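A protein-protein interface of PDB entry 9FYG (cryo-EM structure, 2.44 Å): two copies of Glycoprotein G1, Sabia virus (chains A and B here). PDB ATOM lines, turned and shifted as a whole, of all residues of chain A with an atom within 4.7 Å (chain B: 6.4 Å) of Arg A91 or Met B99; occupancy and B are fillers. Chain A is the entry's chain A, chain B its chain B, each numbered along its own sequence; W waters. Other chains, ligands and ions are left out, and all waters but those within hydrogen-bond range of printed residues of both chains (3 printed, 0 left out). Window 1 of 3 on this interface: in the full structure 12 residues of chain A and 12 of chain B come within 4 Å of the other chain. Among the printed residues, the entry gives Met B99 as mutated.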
ATOM      1  N   LEU A  68      25.040  33.078  -5.125  1.00  0.00           N
ATOM      2  CA  LEU A  68      25.301  32.004  -4.172  1.00  0.00           C
ATOM      3  C   LEU A  68      26.361  31.037  -4.687  1.00  0.00           C
ATOM      4  O   LEU A  68      27.124  30.472  -3.895  1.00  0.00           O
ATOM      5  CB  LEU A  68      23.999  31.264  -3.862  1.00  0.00           C
ATOM      6  CG  LEU A  68      24.021  30.144  -2.822  1.00  0.00           C
ATOM      7  CD1 LEU A  68      24.310  30.690  -1.429  1.00  0.00           C
ATOM      8  CD2 LEU A  68      22.702  29.388  -2.846  1.00  0.00           C
ATOM      9  N   GLU A  87      20.861  25.297  -3.338  1.00  0.00           N
ATOM     10  CA  GLU A  87      19.615  25.840  -3.878  1.00  0.00           C
ATOM     11  C   GLU A  87      18.413  24.981  -3.492  1.00  0.00           C
ATOM     12  O   GLU A  87      17.330  25.507  -3.216  1.00  0.00           O
ATOM     13  CB  GLU A  87      19.716  25.975  -5.395  1.00  0.00           C
ATOM     14  CG  GLU A  87      20.742  26.991  -5.847  1.00  0.00           C
ATOM     15  CD  GLU A  87      20.967  26.964  -7.340  1.00  0.00           C
ATOM     16  OE1 GLU A  87      19.973  26.894  -8.091  1.00  0.00           O
ATOM     17  OE2 GLU A  87      22.137  27.017  -7.765  1.00  0.00           O
ATOM     18  N   TRP A  88      18.586  23.658  -3.495  1.00  0.00           N
ATOM     19  CA  TRP A  88      17.543  22.745  -3.028  1.00  0.00           C
ATOM     20  C   TRP A  88      17.156  23.053  -1.587  1.00  0.00           C
ATOM     21  O   TRP A  88      15.968  23.083  -1.245  1.00  0.00           O
ATOM     22  CB  TRP A  88      18.031  21.298  -3.172  1.00  0.00           C
ATOM     23  CG  TRP A  88      18.102  20.796  -4.600  1.00  0.00           C
ATOM     24  CD1 TRP A  88      19.109  21.009  -5.477  1.00  0.00           C
ATOM     25  CD2 TRP A  88      17.215  19.872  -5.242  1.00  0.00           C
ATOM     26  NE1 TRP A  88      18.871  20.370  -6.661  1.00  0.00           N
ATOM     27  CE2 TRP A  88      17.716  19.649  -6.538  1.00  0.00           C
ATOM     28  CE3 TRP A  88      16.040  19.228  -4.860  1.00  0.00           C
ATOM     29  CZ2 TRP A  88      17.081  18.821  -7.452  1.00  0.00           C
ATOM     30  CZ3 TRP A  88      15.406  18.411  -5.777  1.00  0.00           C
ATOM     31  CH2 TRP A  88      15.926  18.214  -7.055  1.00  0.00           C
ATOM     32  N   ILE A  89      18.149  23.310  -0.735  1.00  0.00           N
ATOM     33  CA  ILE A  89      17.876  23.658   0.658  1.00  0.00           C
ATOM     34  C   ILE A  89      17.157  25.001   0.752  1.00  0.00           C
ATOM     35  O   ILE A  89      16.203  25.153   1.524  1.00  0.00           O
ATOM     36  CB  ILE A  89      19.184  23.654   1.469  1.00  0.00           C
ATOM     37  CG1 ILE A  89      19.644  22.221   1.724  1.00  0.00           C
ATOM     38  CG2 ILE A  89      19.013  24.410   2.779  1.00  0.00           C
ATOM     39  CD1 ILE A  89      21.101  22.114   2.082  1.00  0.00           C
ATOM     40  N   PHE A  90      17.601  25.995  -0.023  1.00  0.00           N
ATOM     41  CA  PHE A  90      16.974  27.313   0.041  1.00  0.00           C
ATOM     42  C   PHE A  90      15.528  27.269  -0.445  1.00  0.00           C
ATOM     43  O   PHE A  90      14.674  27.995   0.076  1.00  0.00           O
ATOM     44  CB  PHE A  90      17.784  28.326  -0.767  1.00  0.00           C
ATOM     45  CG  PHE A  90      18.758  29.119   0.057  1.00  0.00           C
ATOM     46  CD1 PHE A  90      18.315  30.091   0.937  1.00  0.00           C
ATOM     47  CD2 PHE A  90      20.119  28.893  -0.050  1.00  0.00           C
ATOM     48  CE1 PHE A  90      19.208  30.821   1.694  1.00  0.00           C
ATOM     49  CE2 PHE A  90      21.018  29.619   0.703  1.00  0.00           C
ATOM     50  CZ  PHE A  90      20.563  30.584   1.577  1.00  0.00           C
ATOM     51  N   ARG A  91      15.239  26.443  -1.452  1.00  0.00           N
ATOM     52  CA  ARG A  91      13.855  26.251  -1.870  1.00  0.00           C
ATOM     53  C   ARG A  91      13.057  25.507  -0.807  1.00  0.00           C
ATOM     54  O   ARG A  91      11.880  25.807  -0.585  1.00  0.00           O
ATOM     55  CB  ARG A  91      13.797  25.502  -3.199  1.00  0.00           C
ATOM     56  CG  ARG A  91      14.262  26.310  -4.387  1.00  0.00           C
ATOM     57  CD  ARG A  91      13.977  25.585  -5.687  1.00  0.00           C
ATOM     58  NE  ARG A  91      15.031  25.815  -6.667  1.00  0.00           N
ATOM     59  CZ  ARG A  91      16.036  24.983  -6.893  1.00  0.00           C
ATOM     60  NH1 ARG A  91      16.144  23.835  -6.244  1.00  0.00           N
ATOM     61  NH2 ARG A  91      16.958  25.308  -7.794  1.00  0.00           N
ATOM     62  N   ALA A  92      13.681  24.528  -0.146  1.00  0.00           N
ATOM     63  CA  ALA A  92      12.995  23.791   0.909  1.00  0.00           C
ATOM     64  C   ALA A  92      12.621  24.692   2.077  1.00  0.00           C
ATOM     65  O   ALA A  92      11.640  24.424   2.780  1.00  0.00           O
ATOM     66  CB  ALA A  92      13.866  22.630   1.387  1.00  0.00           C
ATOM     67  N   LEU A  93      13.376  25.764   2.295  1.00  0.00           N
ATOM     68  CA  LEU A  93      13.076  26.710   3.359  1.00  0.00           C
ATOM     69  C   LEU A  93      12.033  27.741   2.958  1.00  0.00           C
ATOM     70  O   LEU A  93      11.656  28.565   3.797  1.00  0.00           O
ATOM     71  CB  LEU A  93      14.357  27.420   3.803  1.00  0.00           C
ATOM     72  CG  LEU A  93      15.363  26.573   4.584  1.00  0.00           C
ATOM     73  CD1 LEU A  93      16.708  27.266   4.646  1.00  0.00           C
ATOM     74  CD2 LEU A  93      14.843  26.279   5.976  1.00  0.00           C
ATOM     75  N   LYS A  94      11.562  27.707   1.708  1.00  0.00           N
ATOM     76  CA  LYS A  94      10.657  28.722   1.166  1.00  0.00           C
ATOM     77  C   LYS A  94      11.277  30.113   1.275  1.00  0.00           C
ATOM     78  O   LYS A  94      10.590  31.102   1.536  1.00  0.00           O
ATOM     79  CB  LYS A  94       9.290  28.679   1.853  1.00  0.00           C
ATOM     80  CG  LYS A  94       8.556  27.358   1.726  1.00  0.00           C
ATOM     81  CD  LYS A  94       8.165  27.077   0.292  1.00  0.00           C
ATOM     82  CE  LYS A  94       7.281  25.849   0.195  1.00  0.00           C
ATOM     83  NZ  LYS A  94       8.024  24.603   0.505  1.00  0.00           N
ATOM     84  N   PHE A  97      14.509  35.636  -1.434  1.00  0.00           N
ATOM     85  CA  PHE A  97      15.674  36.511  -1.423  1.00  0.00           C
ATOM     86  C   PHE A  97      15.309  37.977  -1.614  1.00  0.00           C
ATOM     87  O   PHE A  97      16.142  38.848  -1.347  1.00  0.00           O
ATOM     88  CB  PHE A  97      16.668  36.072  -2.500  1.00  0.00           C
ATOM     89  CG  PHE A  97      17.350  34.772  -2.197  1.00  0.00           C
ATOM     90  CD1 PHE A  97      18.459  34.731  -1.369  1.00  0.00           C
ATOM     91  CD2 PHE A  97      16.877  33.585  -2.732  1.00  0.00           C
ATOM     92  CE1 PHE A  97      19.085  33.535  -1.085  1.00  0.00           C
ATOM     93  CE2 PHE A  97      17.498  32.385  -2.452  1.00  0.00           C
ATOM     94  CZ  PHE A  97      18.606  32.361  -1.629  1.00  0.00           C
ATOM     95  N   ALA A 184       9.160  20.353  -1.896  1.00  0.00           N
ATOM     96  CA  ALA A 184       9.568  21.750  -1.960  1.00  0.00           C
ATOM     97  C   ALA A 184      10.378  22.076  -3.210  1.00  0.00           C
ATOM     98  O   ALA A 184      10.599  23.258  -3.490  1.00  0.00           O
ATOM     99  CB  ALA A 184      10.371  22.119  -0.717  1.00  0.00           C
ATOM    100  N   ASN A 185      10.816  21.072  -3.963  1.00  0.00           N
ATOM    101  CA  ASN A 185      11.675  21.250  -5.128  1.00  0.00           C
ATOM    102  C   ASN A 185      11.076  20.578  -6.355  1.00  0.00           C
ATOM    103  O   ASN A 185      11.780  19.933  -7.138  1.00  0.00           O
ATOM    104  CB  ASN A 185      13.072  20.701  -4.859  1.00  0.00           C
ATOM    105  CG  ASN A 185      13.929  21.643  -4.043  1.00  0.00           C
ATOM    106  OD1 ASN A 185      14.499  22.593  -4.570  1.00  0.00           O
ATOM    107  ND2 ASN A 185      14.024  21.383  -2.747  1.00  0.00           N
ATOM    108  N   ARG A 188      12.579  20.371 -10.308  1.00  0.00           N
ATOM    109  CA  ARG A 188      14.032  20.449 -10.383  1.00  0.00           C
ATOM    110  C   ARG A 188      14.602  19.052 -10.597  1.00  0.00           C
ATOM    111  O   ARG A 188      14.305  18.130  -9.831  1.00  0.00           O
ATOM    112  CB  ARG A 188      14.596  21.084  -9.115  1.00  0.00           C
ATOM    113  CG  ARG A 188      14.273  22.559  -8.973  1.00  0.00           C
ATOM    114  CD  ARG A 188      14.978  23.369 -10.045  1.00  0.00           C
ATOM    115  NE  ARG A 188      14.392  24.693 -10.216  1.00  0.00           N
ATOM    116  CZ  ARG A 188      14.971  25.686 -10.878  1.00  0.00           C
ATOM    117  NH1 ARG A 188      16.157  25.541 -11.443  1.00  0.00           N
ATOM    118  NH2 ARG A 188      14.343  26.855 -10.973  1.00  0.00           N
ATOM    119  N   ASP B  96      13.817  31.201 -11.782  1.00  0.00           N
ATOM    120  CA  ASP B  96      14.074  31.932 -10.546  1.00  0.00           C
ATOM    121  C   ASP B  96      15.245  32.870 -10.812  1.00  0.00           C
ATOM    122  O   ASP B  96      16.397  32.436 -10.873  1.00  0.00           O
ATOM    123  CB  ASP B  96      14.365  30.976  -9.393  1.00  0.00           C
ATOM    124  CG  ASP B  96      14.723  31.700  -8.111  1.00  0.00           C
ATOM    125  OD1 ASP B  96      14.122  32.757  -7.829  1.00  0.00           O
ATOM    126  OD2 ASP B  96      15.608  31.210  -7.380  1.00  0.00           O
ATOM    127  N   PHE B  97      14.948  34.160 -10.957  1.00  0.00           N
ATOM    128  CA  PHE B  97      15.982  35.134 -11.282  1.00  0.00           C
ATOM    129  C   PHE B  97      16.981  35.342 -10.151  1.00  0.00           C
ATOM    130  O   PHE B  97      18.021  35.967 -10.378  1.00  0.00           O
ATOM    131  CB  PHE B  97      15.339  36.466 -11.666  1.00  0.00           C
ATOM    132  CG  PHE B  97      14.676  36.448 -13.010  1.00  0.00           C
ATOM    133  CD1 PHE B  97      15.416  36.651 -14.163  1.00  0.00           C
ATOM    134  CD2 PHE B  97      13.316  36.213 -13.125  1.00  0.00           C
ATOM    135  CE1 PHE B  97      14.810  36.629 -15.402  1.00  0.00           C
ATOM    136  CE2 PHE B  97      12.706  36.189 -14.361  1.00  0.00           C
ATOM    137  CZ  PHE B  97      13.455  36.400 -15.500  1.00  0.00           C
ATOM    138  N   ASN B  98      16.699  34.834  -8.953  1.00  0.00           N
ATOM    139  CA  ASN B  98      17.636  34.981  -7.846  1.00  0.00           C
ATOM    140  C   ASN B  98      18.734  33.923  -7.889  1.00  0.00           C
ATOM    141  O   ASN B  98      19.897  34.225  -7.603  1.00  0.00           O
ATOM    142  CB  ASN B  98      16.888  34.918  -6.514  1.00  0.00           C
ATOM    143  CG  ASN B  98      15.895  36.051  -6.350  1.00  0.00           C
ATOM    144  OD1 ASN B  98      14.772  35.845  -5.895  1.00  0.00           O
ATOM    145  ND2 ASN B  98      16.306  37.256  -6.720  1.00  0.00           N
ATOM    146  N   MET B  99      18.391  32.685  -8.253  1.00  0.00           N
ATOM    147  CA  MET B  99      19.339  31.581  -8.208  1.00  0.00           C
ATOM    148  C   MET B  99      19.717  31.025  -9.574  1.00  0.00           C
ATOM    149  O   MET B  99      20.782  30.414  -9.695  1.00  0.00           O
ATOM    150  CB  MET B  99      18.784  30.440  -7.340  1.00  0.00           C
ATOM    151  CG  MET B  99      18.621  30.818  -5.874  1.00  0.00           C
ATOM    152  SD  MET B  99      18.452  29.428  -4.738  1.00  0.00           S
ATOM    153  CE  MET B  99      17.005  28.607  -5.391  1.00  0.00           C
ATOM    154  N   ASP B 100      18.885  31.211 -10.593  1.00  0.00           N
ATOM    155  CA  ASP B 100      19.214  30.743 -11.928  1.00  0.00           C
ATOM    156  C   ASP B 100      20.195  31.699 -12.602  1.00  0.00           C
ATOM    157  O   ASP B 100      20.322  32.856 -12.199  1.00  0.00           O
ATOM    158  CB  ASP B 100      17.945  30.598 -12.762  1.00  0.00           C
ATOM    159  CG  ASP B 100      17.082  29.441 -12.312  1.00  0.00           C
ATOM    160  OD1 ASP B 100      17.554  28.636 -11.484  1.00  0.00           O
ATOM    161  OD2 ASP B 100      15.933  29.336 -12.785  1.00  0.00           O
ATOM    162  N   PRO B 101      20.916  31.229 -13.622  1.00  0.00           N
ATOM    163  CA  PRO B 101      21.888  32.099 -14.299  1.00  0.00           C
ATOM    164  C   PRO B 101      21.236  33.333 -14.904  1.00  0.00           C
ATOM    165  O   PRO B 101      20.104  33.290 -15.390  1.00  0.00           O
ATOM    166  CB  PRO B 101      22.478  31.190 -15.383  1.00  0.00           C
ATOM    167  CG  PRO B 101      22.295  29.817 -14.859  1.00  0.00           C
ATOM    168  CD  PRO B 101      21.010  29.836 -14.089  1.00  0.00           C
ATOM    169  N   SER B 127      24.060  25.599 -11.691  1.00  0.00           N
ATOM    170  CA  SER B 127      24.222  24.492 -10.766  1.00  0.00           C
ATOM    171  C   SER B 127      23.965  23.172 -11.484  1.00  0.00           C
ATOM    172  O   SER B 127      23.412  23.132 -12.587  1.00  0.00           O
ATOM    173  CB  SER B 127      23.285  24.646  -9.571  1.00  0.00           C
ATOM    174  OG  SER B 127      21.940  24.391  -9.935  1.00  0.00           O
HETATM  175  O   HOH W   1      13.523  33.962  -3.812  1.00  0.00           O
HETATM  176  O   HOH W   2      22.623  29.856  -7.361  1.00  0.00           O
HETATM  177  O   HOH W   3      22.281  32.718  -6.417  1.00  0.00           O
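Among the printed residues, merely in contact across the chains: Glu A87 with Met B99, Arg A91 with Met B99, Phe A97 with Asn B98 and Phe A97 with Met B99.
Of the 13 printed residues of chain A, 4 touch a printed residue of chain B.
Printed residues of chain A that touch a printed residue of chain B: Glu A87, Arg A91, Phe A97 and Arg A188.
Along chain A the printed residues that touch a printed residue of chain B span positions 87 to 188.
Of the 7 printed residues of chain B, 4 touch a printed residue of chain A.
Hydrophobic or aromatic side chains of chain B that line the printed part of chain A: Met B99.
Among the printed residues, 6 pairs touch across the chains.
The guanidinium group (NH1) of Arg A188 lies within salt-bridge range of the side-chain carboxylate (OD1) of Asp B100, at 3.4 Å.
The side-chain hydroxyl (OG) of Ser B127 sits close to the side-chain carboxylate (OE2) of Glu A87 (3.4 Å).
Of the printed residues of chain B, Glu A87 touches Met B99 and Ser B127.
Printed residues of chain A within 4 Å of Ser B127: Glu A87 (3.2 Å).
Of the printed residues of chain A, Asn B98 touches Phe A97.
Ala A184 touches none of the printed residues of chain B.
Leu A68 touches none of the printed residues of chain B.
The nearest residue of chain B that does not touch Arg A91 is Asp B100 (5.0 Å).
The nearest printed residue of chain B that does not touch Glu A87 is Asp B100 (4.5 Å).
Position printed for both chains: 97.
Water W2 lies within hydrogen-bond range of OE2 of Glu A87 and O of Met B99.
Water W3 bridges O of Asn B98 (3.1 Å) and N of Leu A68 (3.1 Å).
Water W1 bridges the backbone NH of Phe A97 (3.1 Å) and the side-chain amide oxygen of Asn B98 (3.1 Å).
N of Asp B96 sits at hydrogen-bond distance from OD2 of Asp B100, at 3.0 Å.
N of Met B99 sits close to OD2 of Asp B96, 3.3 Å away.
The side-chain carboxylate (OD1) of Asp B96 lies close to the backbone NH (N) of Asn B98, at 3.5 Å.
NH1 of Arg A91 lies within hydrogen-bond range of OD1 of Asn A185 (2.7 Å).
The guanidinium group of Arg A91 lies within salt-bridge range of the side-chain carboxylate of Glu A87.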
